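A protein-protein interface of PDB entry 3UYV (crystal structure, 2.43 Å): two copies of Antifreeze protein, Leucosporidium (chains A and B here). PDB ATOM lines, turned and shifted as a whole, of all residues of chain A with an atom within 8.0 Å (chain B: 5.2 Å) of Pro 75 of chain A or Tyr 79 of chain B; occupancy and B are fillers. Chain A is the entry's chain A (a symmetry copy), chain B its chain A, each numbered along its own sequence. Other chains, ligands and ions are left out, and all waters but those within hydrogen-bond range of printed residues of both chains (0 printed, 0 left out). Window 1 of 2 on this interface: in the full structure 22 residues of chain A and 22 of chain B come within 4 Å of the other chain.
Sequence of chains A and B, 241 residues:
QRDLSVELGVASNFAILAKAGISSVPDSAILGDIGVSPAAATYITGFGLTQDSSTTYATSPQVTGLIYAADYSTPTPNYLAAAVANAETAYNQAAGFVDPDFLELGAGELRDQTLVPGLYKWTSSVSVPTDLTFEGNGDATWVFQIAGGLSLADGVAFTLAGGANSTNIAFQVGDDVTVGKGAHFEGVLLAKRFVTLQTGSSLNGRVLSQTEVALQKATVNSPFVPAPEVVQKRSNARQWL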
ATOM      1  N   VAL A  10     -18.411  15.898 -23.779  1.00  0.00           N
ATOM      2  CA  VAL A  10     -17.417  16.403 -24.721  1.00  0.00           C
ATOM      3  C   VAL A  10     -17.992  17.517 -25.637  1.00  0.00           C
ATOM      4  O   VAL A  10     -17.294  18.431 -26.008  1.00  0.00           O
ATOM      5  CB  VAL A  10     -16.796  15.256 -25.506  1.00  0.00           C
ATOM      6  CG1 VAL A  10     -15.742  15.760 -26.476  1.00  0.00           C
ATOM      7  CG2 VAL A  10     -16.190  14.245 -24.531  1.00  0.00           C
ATOM      8  N   ASN A  13     -16.988  21.119 -25.569  1.00  0.00           N
ATOM      9  CA  ASN A  13     -15.791  21.525 -26.307  1.00  0.00           C
ATOM     10  C   ASN A  13     -16.086  22.229 -27.668  1.00  0.00           C
ATOM     11  O   ASN A  13     -15.160  22.686 -28.326  1.00  0.00           O
ATOM     12  CB  ASN A  13     -14.870  20.305 -26.559  1.00  0.00           C
ATOM     13  CG  ASN A  13     -14.115  19.827 -25.283  1.00  0.00           C
ATOM     14  OD1 ASN A  13     -14.538  20.069 -24.151  1.00  0.00           O
ATOM     15  ND2 ASN A  13     -13.013  19.113 -25.493  1.00  0.00           N
ATOM     16  N   THR A  56      -4.961  16.138 -38.096  1.00  0.00           N
ATOM     17  CA  THR A  56      -5.994  15.637 -37.224  1.00  0.00           C
ATOM     18  C   THR A  56      -7.076  16.722 -37.066  1.00  0.00           C
ATOM     19  O   THR A  56      -8.136  16.507 -36.470  1.00  0.00           O
ATOM     20  CB  THR A  56      -5.406  15.197 -35.838  1.00  0.00           C
ATOM     21  OG1 THR A  56      -5.017  16.342 -35.068  1.00  0.00           O
ATOM     22  CG2 THR A  56      -4.189  14.299 -36.026  1.00  0.00           C
ATOM     23  N   TYR A  68     -12.943  19.799 -36.825  1.00  0.00           N
ATOM     24  CA  TYR A  68     -12.749  18.370 -36.749  1.00  0.00           C
ATOM     25  C   TYR A  68     -13.765  17.644 -37.626  1.00  0.00           C
ATOM     26  O   TYR A  68     -14.946  17.999 -37.618  1.00  0.00           O
ATOM     27  CB  TYR A  68     -12.907  17.919 -35.298  1.00  0.00           C
ATOM     28  CG  TYR A  68     -11.832  18.442 -34.371  1.00  0.00           C
ATOM     29  CD1 TYR A  68     -10.543  17.911 -34.395  1.00  0.00           C
ATOM     30  CD2 TYR A  68     -12.115  19.438 -33.443  1.00  0.00           C
ATOM     31  CE1 TYR A  68      -9.544  18.378 -33.514  1.00  0.00           C
ATOM     32  CE2 TYR A  68     -11.130  19.910 -32.569  1.00  0.00           C
ATOM     33  CZ  TYR A  68      -9.848  19.382 -32.616  1.00  0.00           C
ATOM     34  OH  TYR A  68      -8.874  19.860 -31.749  1.00  0.00           O
ATOM     35  N   ALA A  69     -13.307  16.637 -38.374  1.00  0.00           N
ATOM     36  CA  ALA A  69     -14.164  15.871 -39.244  1.00  0.00           C
ATOM     37  C   ALA A  69     -13.913  14.399 -38.919  1.00  0.00           C
ATOM     38  O   ALA A  69     -12.827  14.061 -38.441  1.00  0.00           O
ATOM     39  CB  ALA A  69     -13.846  16.171 -40.671  1.00  0.00           C
ATOM     40  N   TYR A  72     -10.716  12.515 -40.207  1.00  0.00           N
ATOM     41  CA  TYR A  72      -9.388  12.998 -39.824  1.00  0.00           C
ATOM     42  C   TYR A  72      -8.553  11.928 -39.045  1.00  0.00           C
ATOM     43  O   TYR A  72      -9.087  10.903 -38.603  1.00  0.00           O
ATOM     44  CB  TYR A  72      -9.505  14.308 -39.042  1.00  0.00           C
ATOM     45  CG  TYR A  72      -9.832  15.506 -39.890  1.00  0.00           C
ATOM     46  CD1 TYR A  72      -9.755  15.458 -41.303  1.00  0.00           C
ATOM     47  CD2 TYR A  72     -10.203  16.703 -39.299  1.00  0.00           C
ATOM     48  CE1 TYR A  72     -10.070  16.601 -42.109  1.00  0.00           C
ATOM     49  CE2 TYR A  72     -10.532  17.821 -40.071  1.00  0.00           C
ATOM     50  CZ  TYR A  72     -10.466  17.775 -41.465  1.00  0.00           C
ATOM     51  OH  TYR A  72     -10.778  18.914 -42.166  1.00  0.00           O
ATOM     52  N   SER A  73      -7.255  12.160 -38.900  1.00  0.00           N
ATOM     53  CA  SER A  73      -6.350  11.171 -38.281  1.00  0.00           C
ATOM     54  C   SER A  73      -6.563  10.987 -36.753  1.00  0.00           C
ATOM     55  O   SER A  73      -6.906  11.944 -36.057  1.00  0.00           O
ATOM     56  CB  SER A  73      -4.895  11.607 -38.519  1.00  0.00           C
ATOM     57  OG  SER A  73      -4.541  11.546 -39.905  1.00  0.00           O
ATOM     58  N   THR A  74      -6.304   9.768 -36.248  1.00  0.00           N
ATOM     59  CA  THR A  74      -6.435   9.385 -34.820  1.00  0.00           C
ATOM     60  C   THR A  74      -5.796  10.424 -33.946  1.00  0.00           C
ATOM     61  O   THR A  74      -4.750  10.945 -34.334  1.00  0.00           O
ATOM     62  CB  THR A  74      -5.799   7.996 -34.550  1.00  0.00           C
ATOM     63  OG1 THR A  74      -6.233   7.049 -35.573  1.00  0.00           O
ATOM     64  CG2 THR A  74      -6.212   7.445 -33.146  1.00  0.00           C
ATOM     65  N   PRO A  75      -6.421  10.767 -32.789  1.00  0.00           N
ATOM     66  CA  PRO A  75      -7.681  10.208 -32.253  1.00  0.00           C
ATOM     67  C   PRO A  75      -8.954  11.005 -32.546  1.00  0.00           C
ATOM     68  O   PRO A  75      -9.959  10.812 -31.813  1.00  0.00           O
ATOM     69  CB  PRO A  75      -7.444  10.251 -30.748  1.00  0.00           C
ATOM     70  CG  PRO A  75      -6.643  11.503 -30.570  1.00  0.00           C
ATOM     71  CD  PRO A  75      -5.745  11.601 -31.777  1.00  0.00           C
ATOM     72  N   THR A  76      -8.952  11.856 -33.583  1.00  0.00           N
ATOM     73  CA  THR A  76     -10.165  12.686 -33.855  1.00  0.00           C
ATOM     74  C   THR A  76     -11.465  11.855 -34.014  1.00  0.00           C
ATOM     75  O   THR A  76     -12.487  12.173 -33.388  1.00  0.00           O
ATOM     76  CB  THR A  76      -9.992  13.654 -35.038  1.00  0.00           C
ATOM     77  OG1 THR A  76      -8.920  14.565 -34.762  1.00  0.00           O
ATOM     78  CG2 THR A  76     -11.267  14.428 -35.282  1.00  0.00           C
ATOM     79  N   PRO A  77     -11.436  10.790 -34.818  1.00  0.00           N
ATOM     80  CA  PRO A  77     -12.674  10.029 -34.921  1.00  0.00           C
ATOM     81  C   PRO A  77     -13.345   9.698 -33.586  1.00  0.00           C
ATOM     82  O   PRO A  77     -14.582   9.816 -33.497  1.00  0.00           O
ATOM     83  CB  PRO A  77     -12.253   8.757 -35.665  1.00  0.00           C
ATOM     84  CG  PRO A  77     -11.090   9.209 -36.538  1.00  0.00           C
ATOM     85  CD  PRO A  77     -10.435  10.374 -35.825  1.00  0.00           C
ATOM     86  N   ASN A  78     -12.568   9.309 -32.565  1.00  0.00           N
ATOM     87  CA  ASN A  78     -13.151   8.894 -31.285  1.00  0.00           C
ATOM     88  C   ASN A  78     -13.425  10.066 -30.370  1.00  0.00           C
ATOM     89  O   ASN A  78     -14.293   9.996 -29.518  1.00  0.00           O
ATOM     90  CB  ASN A  78     -12.220   7.926 -30.536  1.00  0.00           C
ATOM     91  CG  ASN A  78     -12.222   6.516 -31.131  1.00  0.00           C
ATOM     92  OD1 ASN A  78     -13.283   5.981 -31.526  1.00  0.00           O
ATOM     93  ND2 ASN A  78     -11.014   5.913 -31.215  1.00  0.00           N
ATOM     94  N   TYR A  79     -12.600  11.097 -30.478  1.00  0.00           N
ATOM     95  CA  TYR A  79     -12.894  12.383 -29.914  1.00  0.00           C
ATOM     96  C   TYR A  79     -14.312  12.834 -30.358  1.00  0.00           C
ATOM     97  O   TYR A  79     -15.206  13.042 -29.513  1.00  0.00           O
ATOM     98  CB  TYR A  79     -11.815  13.349 -30.360  1.00  0.00           C
ATOM     99  CG  TYR A  79     -11.939  14.705 -29.716  1.00  0.00           C
ATOM    100  CD1 TYR A  79     -12.101  14.826 -28.331  1.00  0.00           C
ATOM    101  CD2 TYR A  79     -11.885  15.882 -30.488  1.00  0.00           C
ATOM    102  CE1 TYR A  79     -12.234  16.072 -27.735  1.00  0.00           C
ATOM    103  CE2 TYR A  79     -12.013  17.149 -29.877  1.00  0.00           C
ATOM    104  CZ  TYR A  79     -12.201  17.232 -28.520  1.00  0.00           C
ATOM    105  OH  TYR A  79     -12.325  18.466 -27.926  1.00  0.00           O
ATOM    106  N   LEU A  80     -14.535  12.903 -31.672  1.00  0.00           N
ATOM    107  CA  LEU A  80     -15.838  13.277 -32.242  1.00  0.00           C
ATOM    108  C   LEU A  80     -16.993  12.366 -31.881  1.00  0.00           C
ATOM    109  O   LEU A  80     -18.090  12.869 -31.644  1.00  0.00           O
ATOM    110  CB  LEU A  80     -15.751  13.384 -33.768  1.00  0.00           C
ATOM    111  CG  LEU A  80     -14.936  14.532 -34.314  1.00  0.00           C
ATOM    112  CD1 LEU A  80     -14.557  14.224 -35.745  1.00  0.00           C
ATOM    113  CD2 LEU A  80     -15.731  15.845 -34.204  1.00  0.00           C
ATOM    114  N   ALA A  81     -16.784  11.045 -31.863  1.00  0.00           N
ATOM    115  CA  ALA A  81     -17.877  10.091 -31.614  1.00  0.00           C
ATOM    116  C   ALA A  81     -18.435  10.283 -30.215  1.00  0.00           C
ATOM    117  O   ALA A  81     -19.649  10.222 -29.966  1.00  0.00           O
ATOM    118  CB  ALA A  81     -17.388   8.672 -31.789  1.00  0.00           C
ATOM    119  N   ALA A  82     -17.538  10.533 -29.280  1.00  0.00           N
ATOM    120  CA  ALA A  82     -17.937  10.808 -27.940  1.00  0.00           C
ATOM    121  C   ALA A  82     -18.703  12.151 -27.832  1.00  0.00           C
ATOM    122  O   ALA A  82     -19.726  12.235 -27.115  1.00  0.00           O
ATOM    123  CB  ALA A  82     -16.709  10.808 -27.091  1.00  0.00           C
ATOM    124  N   PRO A 228      -6.798  21.775 -19.981  1.00  0.00           N
ATOM    125  CA  PRO A 228      -6.489  20.651 -19.075  1.00  0.00           C
ATOM    126  C   PRO A 228      -5.026  20.786 -18.649  1.00  0.00           C
ATOM    127  O   PRO A 228      -4.153  20.897 -19.524  1.00  0.00           O
ATOM    128  CB  PRO A 228      -6.672  19.412 -19.974  1.00  0.00           C
ATOM    129  CG  PRO A 228      -6.505  19.944 -21.411  1.00  0.00           C
ATOM    130  CD  PRO A 228      -7.113  21.313 -21.360  1.00  0.00           C
ATOM    131  N   VAL B  10     -15.732   7.882 -22.140  1.00  0.00           N
ATOM    132  CA  VAL B  10     -14.550   7.738 -22.985  1.00  0.00           C
ATOM    133  C   VAL B  10     -13.550   6.695 -22.420  1.00  0.00           C
ATOM    134  O   VAL B  10     -12.892   6.005 -23.164  1.00  0.00           O
ATOM    135  CB  VAL B  10     -13.908   9.094 -23.239  1.00  0.00           C
ATOM    136  CG1 VAL B  10     -12.690   8.967 -24.137  1.00  0.00           C
ATOM    137  CG2 VAL B  10     -14.942  10.034 -23.864  1.00  0.00           C
ATOM    138  N   ASN B  13     -12.738   3.394 -23.982  1.00  0.00           N
ATOM    139  CA  ASN B  13     -11.738   3.353 -25.049  1.00  0.00           C
ATOM    140  C   ASN B  13     -10.338   2.832 -24.596  1.00  0.00           C
ATOM    141  O   ASN B  13      -9.454   2.676 -25.428  1.00  0.00           O
ATOM    142  CB  ASN B  13     -11.573   4.753 -25.691  1.00  0.00           C
ATOM    143  CG  ASN B  13     -12.766   5.158 -26.606  1.00  0.00           C
ATOM    144  OD1 ASN B  13     -13.885   4.660 -26.470  1.00  0.00           O
ATOM    145  ND2 ASN B  13     -12.511   6.098 -27.512  1.00  0.00           N
ATOM    146  N   PHE B  14     -10.164   2.553 -23.297  1.00  0.00           N
ATOM    147  CA  PHE B  14      -8.851   2.271 -22.738  1.00  0.00           C
ATOM    148  C   PHE B  14      -8.707   0.933 -22.005  1.00  0.00           C
ATOM    149  O   PHE B  14      -9.490   0.618 -21.144  1.00  0.00           O
ATOM    150  CB  PHE B  14      -8.454   3.402 -21.782  1.00  0.00           C
ATOM    151  CG  PHE B  14      -8.133   4.703 -22.486  1.00  0.00           C
ATOM    152  CD1 PHE B  14      -9.141   5.656 -22.726  1.00  0.00           C
ATOM    153  CD2 PHE B  14      -6.859   4.965 -22.924  1.00  0.00           C
ATOM    154  CE1 PHE B  14      -8.881   6.856 -23.387  1.00  0.00           C
ATOM    155  CE2 PHE B  14      -6.560   6.176 -23.586  1.00  0.00           C
ATOM    156  CZ  PHE B  14      -7.596   7.131 -23.823  1.00  0.00           C
ATOM    157  N   ASP B  33      -5.962   0.443 -25.955  1.00  0.00           N
ATOM    158  CA  ASP B  33      -5.169   1.660 -25.776  1.00  0.00           C
ATOM    159  C   ASP B  33      -4.778   1.890 -24.323  1.00  0.00           C
ATOM    160  O   ASP B  33      -5.438   1.423 -23.400  1.00  0.00           O
ATOM    161  CB  ASP B  33      -5.953   2.896 -26.234  1.00  0.00           C
ATOM    162  CG  ASP B  33      -6.323   2.858 -27.707  1.00  0.00           C
ATOM    163  OD1 ASP B  33      -5.584   2.264 -28.512  1.00  0.00           O
ATOM    164  OD2 ASP B  33      -7.381   3.419 -28.060  1.00  0.00           O
ATOM    165  N   THR B  56       0.474  12.568 -32.206  1.00  0.00           N
ATOM    166  CA  THR B  56      -0.644  12.710 -31.308  1.00  0.00           C
ATOM    167  C   THR B  56      -0.774  11.424 -30.470  1.00  0.00           C
ATOM    168  O   THR B  56      -1.575  11.330 -29.536  1.00  0.00           O
ATOM    169  CB  THR B  56      -1.965  13.029 -32.091  1.00  0.00           C
ATOM    170  OG1 THR B  56      -2.418  11.874 -32.810  1.00  0.00           O
ATOM    171  CG2 THR B  56      -1.748  14.166 -33.083  1.00  0.00           C
ATOM    172  N   TYR B  68      -1.427   7.265 -25.351  1.00  0.00           N
ATOM    173  CA  TYR B  68      -1.745   8.673 -25.325  1.00  0.00           C
ATOM    174  C   TYR B  68      -1.217   9.318 -24.047  1.00  0.00           C
ATOM    175  O   TYR B  68      -1.361   8.743 -22.965  1.00  0.00           O
ATOM    176  CB  TYR B  68      -3.261   8.846 -25.399  1.00  0.00           C
ATOM    177  CG  TYR B  68      -3.867   8.401 -26.712  1.00  0.00           C
ATOM    178  CD1 TYR B  68      -3.722   9.170 -27.866  1.00  0.00           C
ATOM    179  CD2 TYR B  68      -4.618   7.234 -26.790  1.00  0.00           C
ATOM    180  CE1 TYR B  68      -4.309   8.772 -29.087  1.00  0.00           C
ATOM    181  CE2 TYR B  68      -5.197   6.828 -27.997  1.00  0.00           C
ATOM    182  CZ  TYR B  68      -5.033   7.597 -29.140  1.00  0.00           C
ATOM    183  OH  TYR B  68      -5.607   7.185 -30.335  1.00  0.00           O
ATOM    184  N   PRO B  75      -5.948  16.629 -31.030  1.00  0.00           N
ATOM    185  CA  PRO B  75      -6.794  16.838 -29.836  1.00  0.00           C
ATOM    186  C   PRO B  75      -6.578  15.866 -28.675  1.00  0.00           C
ATOM    187  O   PRO B  75      -7.498  15.739 -27.824  1.00  0.00           O
ATOM    188  CB  PRO B  75      -8.198  16.601 -30.381  1.00  0.00           C
ATOM    189  CG  PRO B  75      -7.986  15.518 -31.393  1.00  0.00           C
ATOM    190  CD  PRO B  75      -6.646  15.791 -32.026  1.00  0.00           C
ATOM    191  N   THR B  76      -5.411  15.208 -28.597  1.00  0.00           N
ATOM    192  CA  THR B  76      -5.197  14.213 -27.505  1.00  0.00           C
ATOM    193  C   THR B  76      -5.433  14.790 -26.083  1.00  0.00           C
ATOM    194  O   THR B  76      -6.152  14.182 -25.277  1.00  0.00           O
ATOM    195  CB  THR B  76      -3.837  13.500 -27.582  1.00  0.00           C
ATOM    196  OG1 THR B  76      -3.739  12.783 -28.820  1.00  0.00           O
ATOM    197  CG2 THR B  76      -3.672  12.542 -26.426  1.00  0.00           C
ATOM    198  N   PRO B  77      -4.859  15.954 -25.774  1.00  0.00           N
ATOM    199  CA  PRO B  77      -5.123  16.465 -24.436  1.00  0.00           C
ATOM    200  C   PRO B  77      -6.593  16.441 -24.011  1.00  0.00           C
ATOM    201  O   PRO B  77      -6.871  16.071 -22.854  1.00  0.00           O
ATOM    202  CB  PRO B  77      -4.580  17.898 -24.486  1.00  0.00           C
ATOM    203  CG  PRO B  77      -3.446  17.827 -25.501  1.00  0.00           C
ATOM    204  CD  PRO B  77      -3.793  16.713 -26.466  1.00  0.00           C
ATOM    205  N   ASN B  78      -7.519  16.805 -24.910  1.00  0.00           N
ATOM    206  CA  ASN B  78      -8.938  16.887 -24.544  1.00  0.00           C
ATOM    207  C   ASN B  78      -9.639  15.554 -24.657  1.00  0.00           C
ATOM    208  O   ASN B  78     -10.626  15.315 -23.984  1.00  0.00           O
ATOM    209  CB  ASN B  78      -9.686  17.886 -25.443  1.00  0.00           C
ATOM    210  CG  ASN B  78      -9.388  19.345 -25.092  1.00  0.00           C
ATOM    211  OD1 ASN B  78      -9.296  19.720 -23.901  1.00  0.00           O
ATOM    212  ND2 ASN B  78      -9.214  20.177 -26.143  1.00  0.00           N
ATOM    213  N   TYR B  79      -9.190  14.733 -25.597  1.00  0.00           N
ATOM    214  CA  TYR B  79      -9.535  13.342 -25.635  1.00  0.00           C
ATOM    215  C   TYR B  79      -9.265  12.700 -24.247  1.00  0.00           C
ATOM    216  O   TYR B  79     -10.196  12.190 -23.592  1.00  0.00           O
ATOM    217  CB  TYR B  79      -8.730  12.689 -26.740  1.00  0.00           C
ATOM    218  CG  TYR B  79      -9.108  11.249 -26.971  1.00  0.00           C
ATOM    219  CD1 TYR B  79     -10.449  10.878 -27.119  1.00  0.00           C
ATOM    220  CD2 TYR B  79      -8.124  10.245 -27.052  1.00  0.00           C
ATOM    221  CE1 TYR B  79     -10.804   9.553 -27.314  1.00  0.00           C
ATOM    222  CE2 TYR B  79      -8.489   8.897 -27.258  1.00  0.00           C
ATOM    223  CZ  TYR B  79      -9.815   8.562 -27.369  1.00  0.00           C
ATOM    224  OH  TYR B  79     -10.169   7.248 -27.571  1.00  0.00           O
ATOM    225  N   LEU B  80      -8.023  12.801 -23.772  1.00  0.00           N
ATOM    226  CA  LEU B  80      -7.626  12.277 -22.457  1.00  0.00           C
ATOM    227  C   LEU B  80      -8.354  12.875 -21.270  1.00  0.00           C
ATOM    228  O   LEU B  80      -8.675  12.136 -20.341  1.00  0.00           O
ATOM    229  CB  LEU B  80      -6.117  12.434 -22.242  1.00  0.00           C
ATOM    230  CG  LEU B  80      -5.225  11.570 -23.100  1.00  0.00           C
ATOM    231  CD1 LEU B  80      -3.838  12.171 -23.122  1.00  0.00           C
ATOM    232  CD2 LEU B  80      -5.213  10.127 -22.566  1.00  0.00           C
ATOM    233  N   ALA B  81      -8.591  14.190 -21.263  1.00  0.00           N
ATOM    234  CA  ALA B  81      -9.208  14.860 -20.107  1.00  0.00           C
ATOM    235  C   ALA B  81     -10.619  14.341 -19.888  1.00  0.00           C
ATOM    236  O   ALA B  81     -11.081  14.124 -18.758  1.00  0.00           O
ATOM    237  CB  ALA B  81      -9.232  16.358 -20.315  1.00  0.00           C
ATOM    238  N   ALA B  82     -11.316  14.125 -20.986  1.00  0.00           N
ATOM    239  CA  ALA B  82     -12.625  13.566 -20.922  1.00  0.00           C
ATOM    240  C   ALA B  82     -12.601  12.100 -20.421  1.00  0.00           C
ATOM    241  O   ALA B  82     -13.456  11.705 -19.595  1.00  0.00           O
ATOM    242  CB  ALA B  82     -13.232  13.670 -22.283  1.00  0.00           C
ATOM    243  N   ALA B  83     -11.687  11.280 -20.937  1.00  0.00           N
ATOM    244  CA  ALA B  83     -11.517   9.892 -20.459  1.00  0.00           C
ATOM    245  C   ALA B  83     -11.281   9.879 -18.957  1.00  0.00           C
ATOM    246  O   ALA B  83     -11.968   9.200 -18.198  1.00  0.00           O
ATOM    247  CB  ALA B  83     -10.348   9.265 -21.155  1.00  0.00           C
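Printed residues of chain B within 4 Å of Asn 13 of chain A: Asn 78.
Ser 73 of chain A touches none of the printed residues of chain B.
Pro 75 of chain A touches just these residues of chain B: Thr 56, Tyr 68, Thr 76 and Tyr 79.
Of the printed residues of chain B, Pro 228 of chain A touches Asn 78 (3.7 Å) and Ala 81 (3.9996 Å).
Tyr 79 of chain B touches three residues of chain A.
Of the printed residues of chain A, Ala 81 of chain B touches Pro 228 (3.9996 Å).
The nearest residue of chain A that does not touch Tyr 79 of chain B is Asn 13 of chain A (5.8 Å).
The nearest printed residue of chain B that does not touch Tyr 79 of chain A is Asn 13 of chain B (5.8 Å).
Of the 17 printed residues of chain A, 11 touch a printed residue of chain B.
Printed residues of chain B that touch a printed residue of chain A: Val 10, Asn 13, Thr 56, Tyr 68, Pro 75, Thr 76, Asn 78, Tyr 79, Ala 81 and Ala 82.
Hydrophobic or aromatic side chains of chain B that line the printed part of chain A: Val 10, Tyr 68, Pro 75, Tyr 79, Ala 81 and Ala 82.
Among the printed residues, 20 pairs touch across the chains.
Among the printed residues, no Asp or Glu carboxylate lies within 4 Å of a Lys or Arg side-chain nitrogen of the other chain.
Among the printed residues, merely in contact across the chains: Thr 74 of chain A with Tyr 68 of chain B (2.9 Å), Pro 75 of chain A with Thr 56 of chain B (3.5 Å), Thr 56 of chain A with Pro 75 of chain B (3.5 Å), Asn 78 of chain A with Asn 13 of chain B (3.5 Å), Asn 13 of chain A with Asn 78 of chain B (3.5 Å), Pro 75 of chain A with Tyr 68 of chain B (3.6 Å), Tyr 68 of chain A with Pro 75 of chain B (3.6 Å), Thr 76 of chain A with Pro 75 of chain B (3.6 Å), Pro 75 of chain A with Thr 76 of chain B (3.6 Å), Asn 78 of chain A with Tyr 79 of chain B (3.7 Å), Tyr 79 of chain A with Asn 78 of chain B (3.7 Å), Pro 228 of chain A with Asn 78 of chain B (3.7 Å), Tyr 79 of chain A with Pro 75 of chain B (3.8 Å), Pro 75 of chain A with Tyr 79 of chain B (3.8 Å), Val 10 of chain A with Ala 82 of chain B (3.8 Å), Ala 82 of chain A with Val 10 of chain B (3.8 Å), Thr 56 of chain A with Thr 56 of chain B (3.8 Å), Tyr 79 of chain A with Tyr 79 of chain B (3.95 Å) and Pro 228 of chain A with Ala 81 of chain B (3.9996 Å).
The side-chain hydroxyl (OG1) of Thr 76 of chain A sits at hydrogen-bond distance from the backbone carbonyl oxygen (O) of Thr 56 of chain A (2.7 Å).
OH of Tyr 79 of chain A sits at hydrogen-bond distance from ND2 of Asn 13 of chain A, at 2.6 Å.
OH of Tyr 79 of chain B is in hydrogen-bond range of ND2 of Asn 13 of chain B (2.6 Å).
The backbone carbonyl oxygen (O) of Thr 56 of chain B sits at hydrogen-bond distance from the side-chain hydroxyl (OG1) of Thr 76 of chain B, 2.7 Å away.
O of Thr 74 of chain A sits at hydrogen-bond distance from OG1 of Thr 56 of chain B, at 2.9 Å.
Val 10 of chain A touches Ala 82 of chain B, and with the chains exchanged Ala 82 of chain A touches Val 10 of chain B.
Asn 13 of chain A touches Asn 78 of chain B, and with the chains exchanged Asn 78 of chain A touches Asn 13 of chain B.
Thr 56 of chain A touches Pro 75 of chain B, and with the chains exchanged Pro 75 of chain A touches Thr 56 of chain B.
Pro 75 of chain A touches Tyr 79 of chain B, and with the chains exchanged Tyr 79 of chain A touches Pro 75 of chain B.
12 positions are printed for both chains.
Of the 20 pairs that touch across the chains among the printed residues, 16 have their exchanged pair printed and touching as well.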
